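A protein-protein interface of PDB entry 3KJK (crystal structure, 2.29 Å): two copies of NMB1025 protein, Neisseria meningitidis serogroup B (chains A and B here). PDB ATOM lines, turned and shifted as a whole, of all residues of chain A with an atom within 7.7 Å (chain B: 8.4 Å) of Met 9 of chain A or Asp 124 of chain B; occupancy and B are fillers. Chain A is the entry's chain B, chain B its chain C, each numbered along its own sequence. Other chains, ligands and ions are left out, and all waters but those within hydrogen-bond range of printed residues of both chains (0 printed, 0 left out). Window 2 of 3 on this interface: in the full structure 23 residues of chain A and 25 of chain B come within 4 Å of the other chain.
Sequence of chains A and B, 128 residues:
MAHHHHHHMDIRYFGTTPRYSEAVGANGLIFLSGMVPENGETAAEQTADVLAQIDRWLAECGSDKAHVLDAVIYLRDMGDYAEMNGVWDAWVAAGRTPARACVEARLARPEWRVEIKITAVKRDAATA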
ATOM      1  N   MET A   9      -4.357  18.305 -20.382  1.00  0.00           N
ATOM      2  CA  MET A   9      -3.828  16.978 -19.930  1.00  0.00           C
ATOM      3  C   MET A   9      -4.519  15.803 -20.640  1.00  0.00           C
ATOM      4  O   MET A   9      -5.033  14.881 -19.994  1.00  0.00           O
ATOM      5  CB  MET A   9      -3.935  16.838 -18.401  1.00  0.00           C
ATOM      6  CG  MET A   9      -3.022  17.768 -17.606  1.00  0.00           C
ATOM      7  SD  MET A   9      -1.127  17.532 -18.024  1.00  0.00           S
ATOM      8  CE  MET A   9      -0.635  16.184 -16.711  1.00  0.00           C
ATOM      9  N   ASP A  10      -4.521  15.843 -21.972  1.00  0.00           N
ATOM     10  CA  ASP A  10      -5.117  14.788 -22.789  1.00  0.00           C
ATOM     11  C   ASP A  10      -4.219  13.558 -22.805  1.00  0.00           C
ATOM     12  O   ASP A  10      -3.002  13.676 -22.944  1.00  0.00           O
ATOM     13  CB  ASP A  10      -5.355  15.283 -24.220  1.00  0.00           C
ATOM     14  CG  ASP A  10      -6.278  16.491 -24.281  1.00  0.00           C
ATOM     15  OD1 ASP A  10      -5.944  17.544 -23.690  1.00  0.00           O
ATOM     16  OD2 ASP A  10      -7.337  16.389 -24.934  1.00  0.00           O
ATOM     17  N   ILE A  11      -4.826  12.381 -22.669  1.00  0.00           N
ATOM     18  CA  ILE A  11      -4.074  11.128 -22.579  1.00  0.00           C
ATOM     19  C   ILE A  11      -4.146  10.304 -23.861  1.00  0.00           C
ATOM     20  O   ILE A  11      -5.237   9.998 -24.343  1.00  0.00           O
ATOM     21  CB  ILE A  11      -4.564  10.233 -21.418  1.00  0.00           C
ATOM     22  CG1 ILE A  11      -4.692  11.030 -20.119  1.00  0.00           C
ATOM     23  CG2 ILE A  11      -3.619   9.048 -21.235  1.00  0.00           C
ATOM     24  CD1 ILE A  11      -5.466  10.295 -19.053  1.00  0.00           C
ATOM     25  N   ARG A  12      -2.976   9.946 -24.391  1.00  0.00           N
ATOM     26  CA  ARG A  12      -2.862   9.041 -25.537  1.00  0.00           C
ATOM     27  C   ARG A  12      -2.386   7.669 -25.073  1.00  0.00           C
ATOM     28  O   ARG A  12      -1.469   7.561 -24.250  1.00  0.00           O
ATOM     29  CB  ARG A  12      -1.883   9.583 -26.586  1.00  0.00           C
ATOM     30  CG  ARG A  12      -2.426  10.695 -27.471  1.00  0.00           C
ATOM     31  CD  ARG A  12      -1.577  10.863 -28.731  1.00  0.00           C
ATOM     32  NE  ARG A  12      -1.680   9.707 -29.628  1.00  0.00           N
ATOM     33  CZ  ARG A  12      -1.031   9.581 -30.788  1.00  0.00           C
ATOM     34  NH1 ARG A  12      -0.213  10.538 -31.217  1.00  0.00           N
ATOM     35  NH2 ARG A  12      -1.200   8.487 -31.522  1.00  0.00           N
ATOM     36  N   GLY A  25       1.018   8.625 -23.143  1.00  0.00           N
ATOM     37  CA  GLY A  25       1.518   9.991 -23.261  1.00  0.00           C
ATOM     38  C   GLY A  25       0.536  11.021 -22.730  1.00  0.00           C
ATOM     39  O   GLY A  25      -0.663  10.944 -22.999  1.00  0.00           O
ATOM     40  N   ALA A  26       1.042  11.983 -21.967  1.00  0.00           N
ATOM     41  CA  ALA A  26       0.218  13.081 -21.482  1.00  0.00           C
ATOM     42  C   ALA A  26       1.050  14.347 -21.425  1.00  0.00           C
ATOM     43  O   ALA A  26       2.166  14.329 -20.906  1.00  0.00           O
ATOM     44  CB  ALA A  26      -0.364  12.758 -20.111  1.00  0.00           C
ATOM     45  N   ASN A  27       0.511  15.433 -21.973  1.00  0.00           N
ATOM     46  CA  ASN A  27       1.171  16.746 -21.955  1.00  0.00           C
ATOM     47  C   ASN A  27       2.668  16.685 -22.291  1.00  0.00           C
ATOM     48  O   ASN A  27       3.510  17.169 -21.528  1.00  0.00           O
ATOM     49  CB  ASN A  27       0.945  17.428 -20.597  1.00  0.00           C
ATOM     50  CG  ASN A  27       1.219  18.926 -20.630  1.00  0.00           C
ATOM     51  OD1 ASN A  27       1.060  19.584 -21.660  1.00  0.00           O
ATOM     52  ND2 ASN A  27       1.627  19.472 -19.490  1.00  0.00           N
ATOM     53  N   GLY A  28       2.989  16.066 -23.424  1.00  0.00           N
ATOM     54  CA  GLY A  28       4.376  15.926 -23.862  1.00  0.00           C
ATOM     55  C   GLY A  28       5.188  14.825 -23.190  1.00  0.00           C
ATOM     56  O   GLY A  28       6.241  14.444 -23.704  1.00  0.00           O
ATOM     57  N   LEU A  29       4.716  14.319 -22.048  1.00  0.00           N
ATOM     58  CA  LEU A  29       5.417  13.260 -21.315  1.00  0.00           C
ATOM     59  C   LEU A  29       5.022  11.877 -21.809  1.00  0.00           C
ATOM     60  O   LEU A  29       3.870  11.657 -22.197  1.00  0.00           O
ATOM     61  CB  LEU A  29       5.125  13.344 -19.815  1.00  0.00           C
ATOM     62  CG  LEU A  29       5.827  14.394 -18.962  1.00  0.00           C
ATOM     63  CD1 LEU A  29       5.181  14.449 -17.589  1.00  0.00           C
ATOM     64  CD2 LEU A  29       7.310  14.081 -18.841  1.00  0.00           C
ATOM     65  N   ALA B  26       1.084  18.172  -8.939  1.00  0.00           N
ATOM     66  CA  ALA B  26       1.776  19.323  -9.534  1.00  0.00           C
ATOM     67  C   ALA B  26       1.559  19.379 -11.038  1.00  0.00           C
ATOM     68  O   ALA B  26       1.752  18.380 -11.732  1.00  0.00           O
ATOM     69  CB  ALA B  26       3.266  19.282  -9.222  1.00  0.00           C
ATOM     70  N   ASN B  27       1.167  20.552 -11.536  1.00  0.00           N
ATOM     71  CA  ASN B  27       0.935  20.772 -12.970  1.00  0.00           C
ATOM     72  C   ASN B  27       0.157  19.636 -13.642  1.00  0.00           C
ATOM     73  O   ASN B  27       0.611  19.049 -14.628  1.00  0.00           O
ATOM     74  CB  ASN B  27       2.261  21.019 -13.698  1.00  0.00           C
ATOM     75  CG  ASN B  27       2.075  21.591 -15.095  1.00  0.00           C
ATOM     76  OD1 ASN B  27       1.068  22.236 -15.393  1.00  0.00           O
ATOM     77  ND2 ASN B  27       3.053  21.355 -15.959  1.00  0.00           N
ATOM     78  N   GLY B  28      -1.005  19.318 -13.082  1.00  0.00           N
ATOM     79  CA  GLY B  28      -1.868  18.281 -13.629  1.00  0.00           C
ATOM     80  C   GLY B  28      -1.485  16.845 -13.307  1.00  0.00           C
ATOM     81  O   GLY B  28      -2.283  15.941 -13.530  1.00  0.00           O
ATOM     82  N   LEU B  29      -0.272  16.635 -12.793  1.00  0.00           N
ATOM     83  CA  LEU B  29       0.232  15.292 -12.487  1.00  0.00           C
ATOM     84  C   LEU B  29      -0.019  14.908 -11.040  1.00  0.00           C
ATOM     85  O   LEU B  29       0.006  15.757 -10.150  1.00  0.00           O
ATOM     86  CB  LEU B  29       1.735  15.188 -12.765  1.00  0.00           C
ATOM     87  CG  LEU B  29       2.184  15.100 -14.219  1.00  0.00           C
ATOM     88  CD1 LEU B  29       3.654  15.473 -14.341  1.00  0.00           C
ATOM     89  CD2 LEU B  29       1.906  13.704 -14.771  1.00  0.00           C
ATOM     90  N   ILE B  30      -0.230  13.614 -10.816  1.00  0.00           N
ATOM     91  CA  ILE B  30      -0.524  13.095  -9.485  1.00  0.00           C
ATOM     92  C   ILE B  30       0.370  11.908  -9.196  1.00  0.00           C
ATOM     93  O   ILE B  30       0.368  10.933  -9.942  1.00  0.00           O
ATOM     94  CB  ILE B  30      -2.001  12.655  -9.359  1.00  0.00           C
ATOM     95  CG1 ILE B  30      -2.947  13.847  -9.558  1.00  0.00           C
ATOM     96  CG2 ILE B  30      -2.248  11.998  -8.000  1.00  0.00           C
ATOM     97  CD1 ILE B  30      -4.375  13.460  -9.897  1.00  0.00           C
ATOM     98  N   GLY B  62      -8.896  14.498  -7.773  1.00  0.00           N
ATOM     99  CA  GLY B  62      -9.590  14.879  -9.006  1.00  0.00           C
ATOM    100  C   GLY B  62      -9.285  13.977 -10.189  1.00  0.00           C
ATOM    101  O   GLY B  62      -9.334  14.415 -11.344  1.00  0.00           O
ATOM    102  N   SER B  63      -8.980  12.714  -9.894  1.00  0.00           N
ATOM    103  CA  SER B  63      -8.661  11.717 -10.910  1.00  0.00           C
ATOM    104  C   SER B  63      -9.463  10.432 -10.696  1.00  0.00           C
ATOM    105  O   SER B  63     -10.307  10.343  -9.792  1.00  0.00           O
ATOM    106  CB  SER B  63      -7.158  11.407 -10.881  1.00  0.00           C
ATOM    107  OG  SER B  63      -6.754  10.667 -12.028  1.00  0.00           O
ATOM    108  N   HIS B  67      -7.681   7.454 -15.747  1.00  0.00           N
ATOM    109  CA  HIS B  67      -6.732   8.548 -15.974  1.00  0.00           C
ATOM    110  C   HIS B  67      -5.376   8.249 -15.339  1.00  0.00           C
ATOM    111  O   HIS B  67      -4.595   9.156 -15.053  1.00  0.00           O
ATOM    112  CB  HIS B  67      -7.304   9.862 -15.447  1.00  0.00           C
ATOM    113  CG  HIS B  67      -8.422  10.402 -16.282  1.00  0.00           C
ATOM    114  ND1 HIS B  67      -9.713   9.930 -16.191  1.00  0.00           N
ATOM    115  CD2 HIS B  67      -8.440  11.371 -17.229  1.00  0.00           C
ATOM    116  CE1 HIS B  67     -10.480  10.585 -17.046  1.00  0.00           C
ATOM    117  NE2 HIS B  67      -9.731  11.463 -17.689  1.00  0.00           N
ATOM    118  N   LEU B  69      -1.630   6.877 -15.553  1.00  0.00           N
ATOM    119  CA  LEU B  69      -0.585   6.853 -16.574  1.00  0.00           C
ATOM    120  C   LEU B  69       0.322   5.652 -16.417  1.00  0.00           C
ATOM    121  O   LEU B  69       0.734   5.045 -17.406  1.00  0.00           O
ATOM    122  CB  LEU B  69       0.276   8.114 -16.487  1.00  0.00           C
ATOM    123  CG  LEU B  69      -0.376   9.478 -16.701  1.00  0.00           C
ATOM    124  CD1 LEU B  69       0.665  10.547 -16.514  1.00  0.00           C
ATOM    125  CD2 LEU B  69      -0.990   9.562 -18.076  1.00  0.00           C
ATOM    126  N   ARG B  96      -8.158   1.989 -21.690  1.00  0.00           N
ATOM    127  CA  ARG B  96      -7.410   3.029 -20.968  1.00  0.00           C
ATOM    128  C   ARG B  96      -6.537   2.409 -19.867  1.00  0.00           C
ATOM    129  O   ARG B  96      -6.444   2.914 -18.740  1.00  0.00           O
ATOM    130  CB  ARG B  96      -8.363   4.101 -20.410  1.00  0.00           C
ATOM    131  CG  ARG B  96      -9.304   4.725 -21.458  1.00  0.00           C
ATOM    132  CD  ARG B  96     -10.255   5.757 -20.871  1.00  0.00           C
ATOM    133  NE  ARG B  96      -9.549   6.917 -20.328  1.00  0.00           N
ATOM    134  CZ  ARG B  96      -9.363   8.070 -20.964  1.00  0.00           C
ATOM    135  NH1 ARG B  96      -9.836   8.252 -22.190  1.00  0.00           N
ATOM    136  NH2 ARG B  96      -8.704   9.049 -20.366  1.00  0.00           N
ATOM    137  N   ALA B 120      -0.629   9.442 -12.037  1.00  0.00           N
ATOM    138  CA  ALA B 120      -1.873   9.724 -12.728  1.00  0.00           C
ATOM    139  C   ALA B 120      -1.968  11.189 -13.176  1.00  0.00           C
ATOM    140  O   ALA B 120      -1.013  11.957 -13.020  1.00  0.00           O
ATOM    141  CB  ALA B 120      -3.047   9.364 -11.830  1.00  0.00           C
ATOM    142  N   VAL B 121      -3.116  11.564 -13.738  1.00  0.00           N
ATOM    143  CA  VAL B 121      -3.393  12.948 -14.130  1.00  0.00           C
ATOM    144  C   VAL B 121      -4.774  13.391 -13.672  1.00  0.00           C
ATOM    145  O   VAL B 121      -5.671  12.578 -13.578  1.00  0.00           O
ATOM    146  CB  VAL B 121      -3.259  13.173 -15.662  1.00  0.00           C
ATOM    147  CG1 VAL B 121      -1.852  12.906 -16.106  1.00  0.00           C
ATOM    148  CG2 VAL B 121      -4.208  12.293 -16.434  1.00  0.00           C
ATOM    149  N   LYS B 122      -4.933  14.680 -13.380  1.00  0.00           N
ATOM    150  CA  LYS B 122      -6.245  15.261 -13.062  1.00  0.00           C
ATOM    151  C   LYS B 122      -7.109  15.302 -14.305  1.00  0.00           C
ATOM    152  O   LYS B 122      -6.580  15.364 -15.410  1.00  0.00           O
ATOM    153  CB  LYS B 122      -6.093  16.697 -12.565  1.00  0.00           C
ATOM    154  CG  LYS B 122      -5.582  16.846 -11.160  1.00  0.00           C
ATOM    155  CD  LYS B 122      -5.751  18.272 -10.675  1.00  0.00           C
ATOM    156  CE  LYS B 122      -7.073  18.448  -9.935  1.00  0.00           C
ATOM    157  NZ  LYS B 122      -7.670  19.797 -10.186  1.00  0.00           N
ATOM    158  N   ARG B 123      -8.429  15.281 -14.128  1.00  0.00           N
ATOM    159  CA  ARG B 123      -9.363  15.573 -15.225  1.00  0.00           C
ATOM    160  C   ARG B 123      -9.343  17.068 -15.544  1.00  0.00           C
ATOM    161  O   ARG B 123      -9.169  17.897 -14.647  1.00  0.00           O
ATOM    162  CB  ARG B 123     -10.794  15.167 -14.866  1.00  0.00           C
ATOM    163  CG  ARG B 123     -11.025  13.687 -14.687  1.00  0.00           C
ATOM    164  CD  ARG B 123     -12.462  13.421 -14.255  1.00  0.00           C
ATOM    165  NE  ARG B 123     -12.501  12.457 -13.161  1.00  0.00           N
ATOM    166  CZ  ARG B 123     -12.662  12.770 -11.878  1.00  0.00           C
ATOM    167  NH1 ARG B 123     -12.663  11.811 -10.968  1.00  0.00           N
ATOM    168  NH2 ARG B 123     -12.830  14.030 -11.500  1.00  0.00           N
ATOM    169  N   ASP B 124      -9.533  17.405 -16.819  1.00  0.00           N
ATOM    170  CA  ASP B 124      -9.592  18.803 -17.254  1.00  0.00           C
ATOM    171  C   ASP B 124     -11.009  19.362 -17.146  1.00  0.00           C
ATOM    172  O   ASP B 124     -11.565  19.460 -16.049  1.00  0.00           O
ATOM    173  CB  ASP B 124      -9.071  18.951 -18.691  1.00  0.00           C
ATOM    174  CG  ASP B 124      -7.546  18.984 -18.771  1.00  0.00           C
ATOM    175  OD1 ASP B 124      -7.020  19.217 -19.882  1.00  0.00           O
ATOM    176  OD2 ASP B 124      -6.870  18.784 -17.737  1.00  0.00           O
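The backbone NH (N) of Met 9 of chain A lies within hydrogen-bond range of the side-chain carboxylate (OD1) of Asp 124 of chain B, at 2.9 Å.
Of chain B, only Asn 27 (3.8 Å), Gly 28 (3.6 Å), Leu 29 (3.9 Å), Val 121 (3.5 Å) and Asp 124 (2.9 Å) come within 4 Å of Met 9 of chain A.
Of the printed residues of chain A, Asp 124 of chain B touches Met 9 (2.9 Å).
Of the printed residues of chain B, Ile 11 of chain A touches His 67, Arg 96 and Val 121.
Printed residues of chain A within 4 Å of His 67 of chain B: Ile 11.
Printed residues of chain A within 4 Å of Arg 96 of chain B: Ile 11 (3.7 Å).
Of the printed residues of chain A, Gly 28 of chain B touches Met 9.
Printed residues of chain A within 4 Å of Asn 27 of chain B: Met 9 (3.8 Å).
Gly 28 of chain A touches none of the printed residues of chain B.
Asp 10 of chain A touches none of the printed residues of chain B.
The nearest residue of chain A that does not touch Asp 124 of chain B is Asp 10 of chain A (4.3 Å).
Leu 29 of chain A touches its own counterpart, Leu 29 of chain B.
Positions printed for both chains: 26, 27, 28 and 29.
Of the 10 pairs that touch across the chains among the printed residues, 1 has its exchanged pair printed and touching as well.
Of the 9 printed residues of chain A, 4 touch a printed residue of chain B.
Printed residues of chain A that touch a printed residue of chain B: Met 9, Ile 11, Ala 26 and Leu 29.
Hydrophobic or aromatic side chains of chain A that line the printed part of chain B: Met 9, Ile 11, Ala 26 and Leu 29.
Among the printed residues, no Asp or Glu carboxylate lies within 4 Å of a Lys or Arg side-chain nitrogen of the other chain.
Met 9 of chain A touches Asn 27 of chain B (CE to O, 3.8 Å).
CE of Met 9 of chain A touches C of Gly 28 of chain B, at 3.6 Å.
Met 9 of chain A touches Leu 29 of chain B.
Met 9 of chain A touches Val 121 of chain B.
CD2 of His 67 of chain B touches CD1 of Ile 11 of chain A, at 3.7 Å.
CD1 of Ile 11 of chain A touches NH2 of Arg 96 of chain B, at 3.7 Å.
Val 121 of chain B touches Ile 11 of chain A (CG2 to CD1, 3.5 Å).
CD2 of Leu 69 of chain B touches CB of Ala 26 of chain A, 3.8 Å away.
Leu 29 of chain A touches Leu 29 of chain B (CD1 to CD1, 3.7 Å).
The side-chain sulfur (SD) of Met 9 of chain A lies close to the side-chain amide nitrogen (ND2) of Asn 27 of chain A (3.7 Å).
The backbone carbonyl oxygen (O) of His 67 of chain B lies within hydrogen-bond range of the backbone NH (N) of Val 121 of chain B (3.1 Å).
N of Lys 122 of chain B lies within hydrogen-bond range of O of Gly 28 of chain B (2.9 Å).
OG of Ser 63 of chain B lies within hydrogen-bond range of O of Val 121 of chain B, 2.7 Å away.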
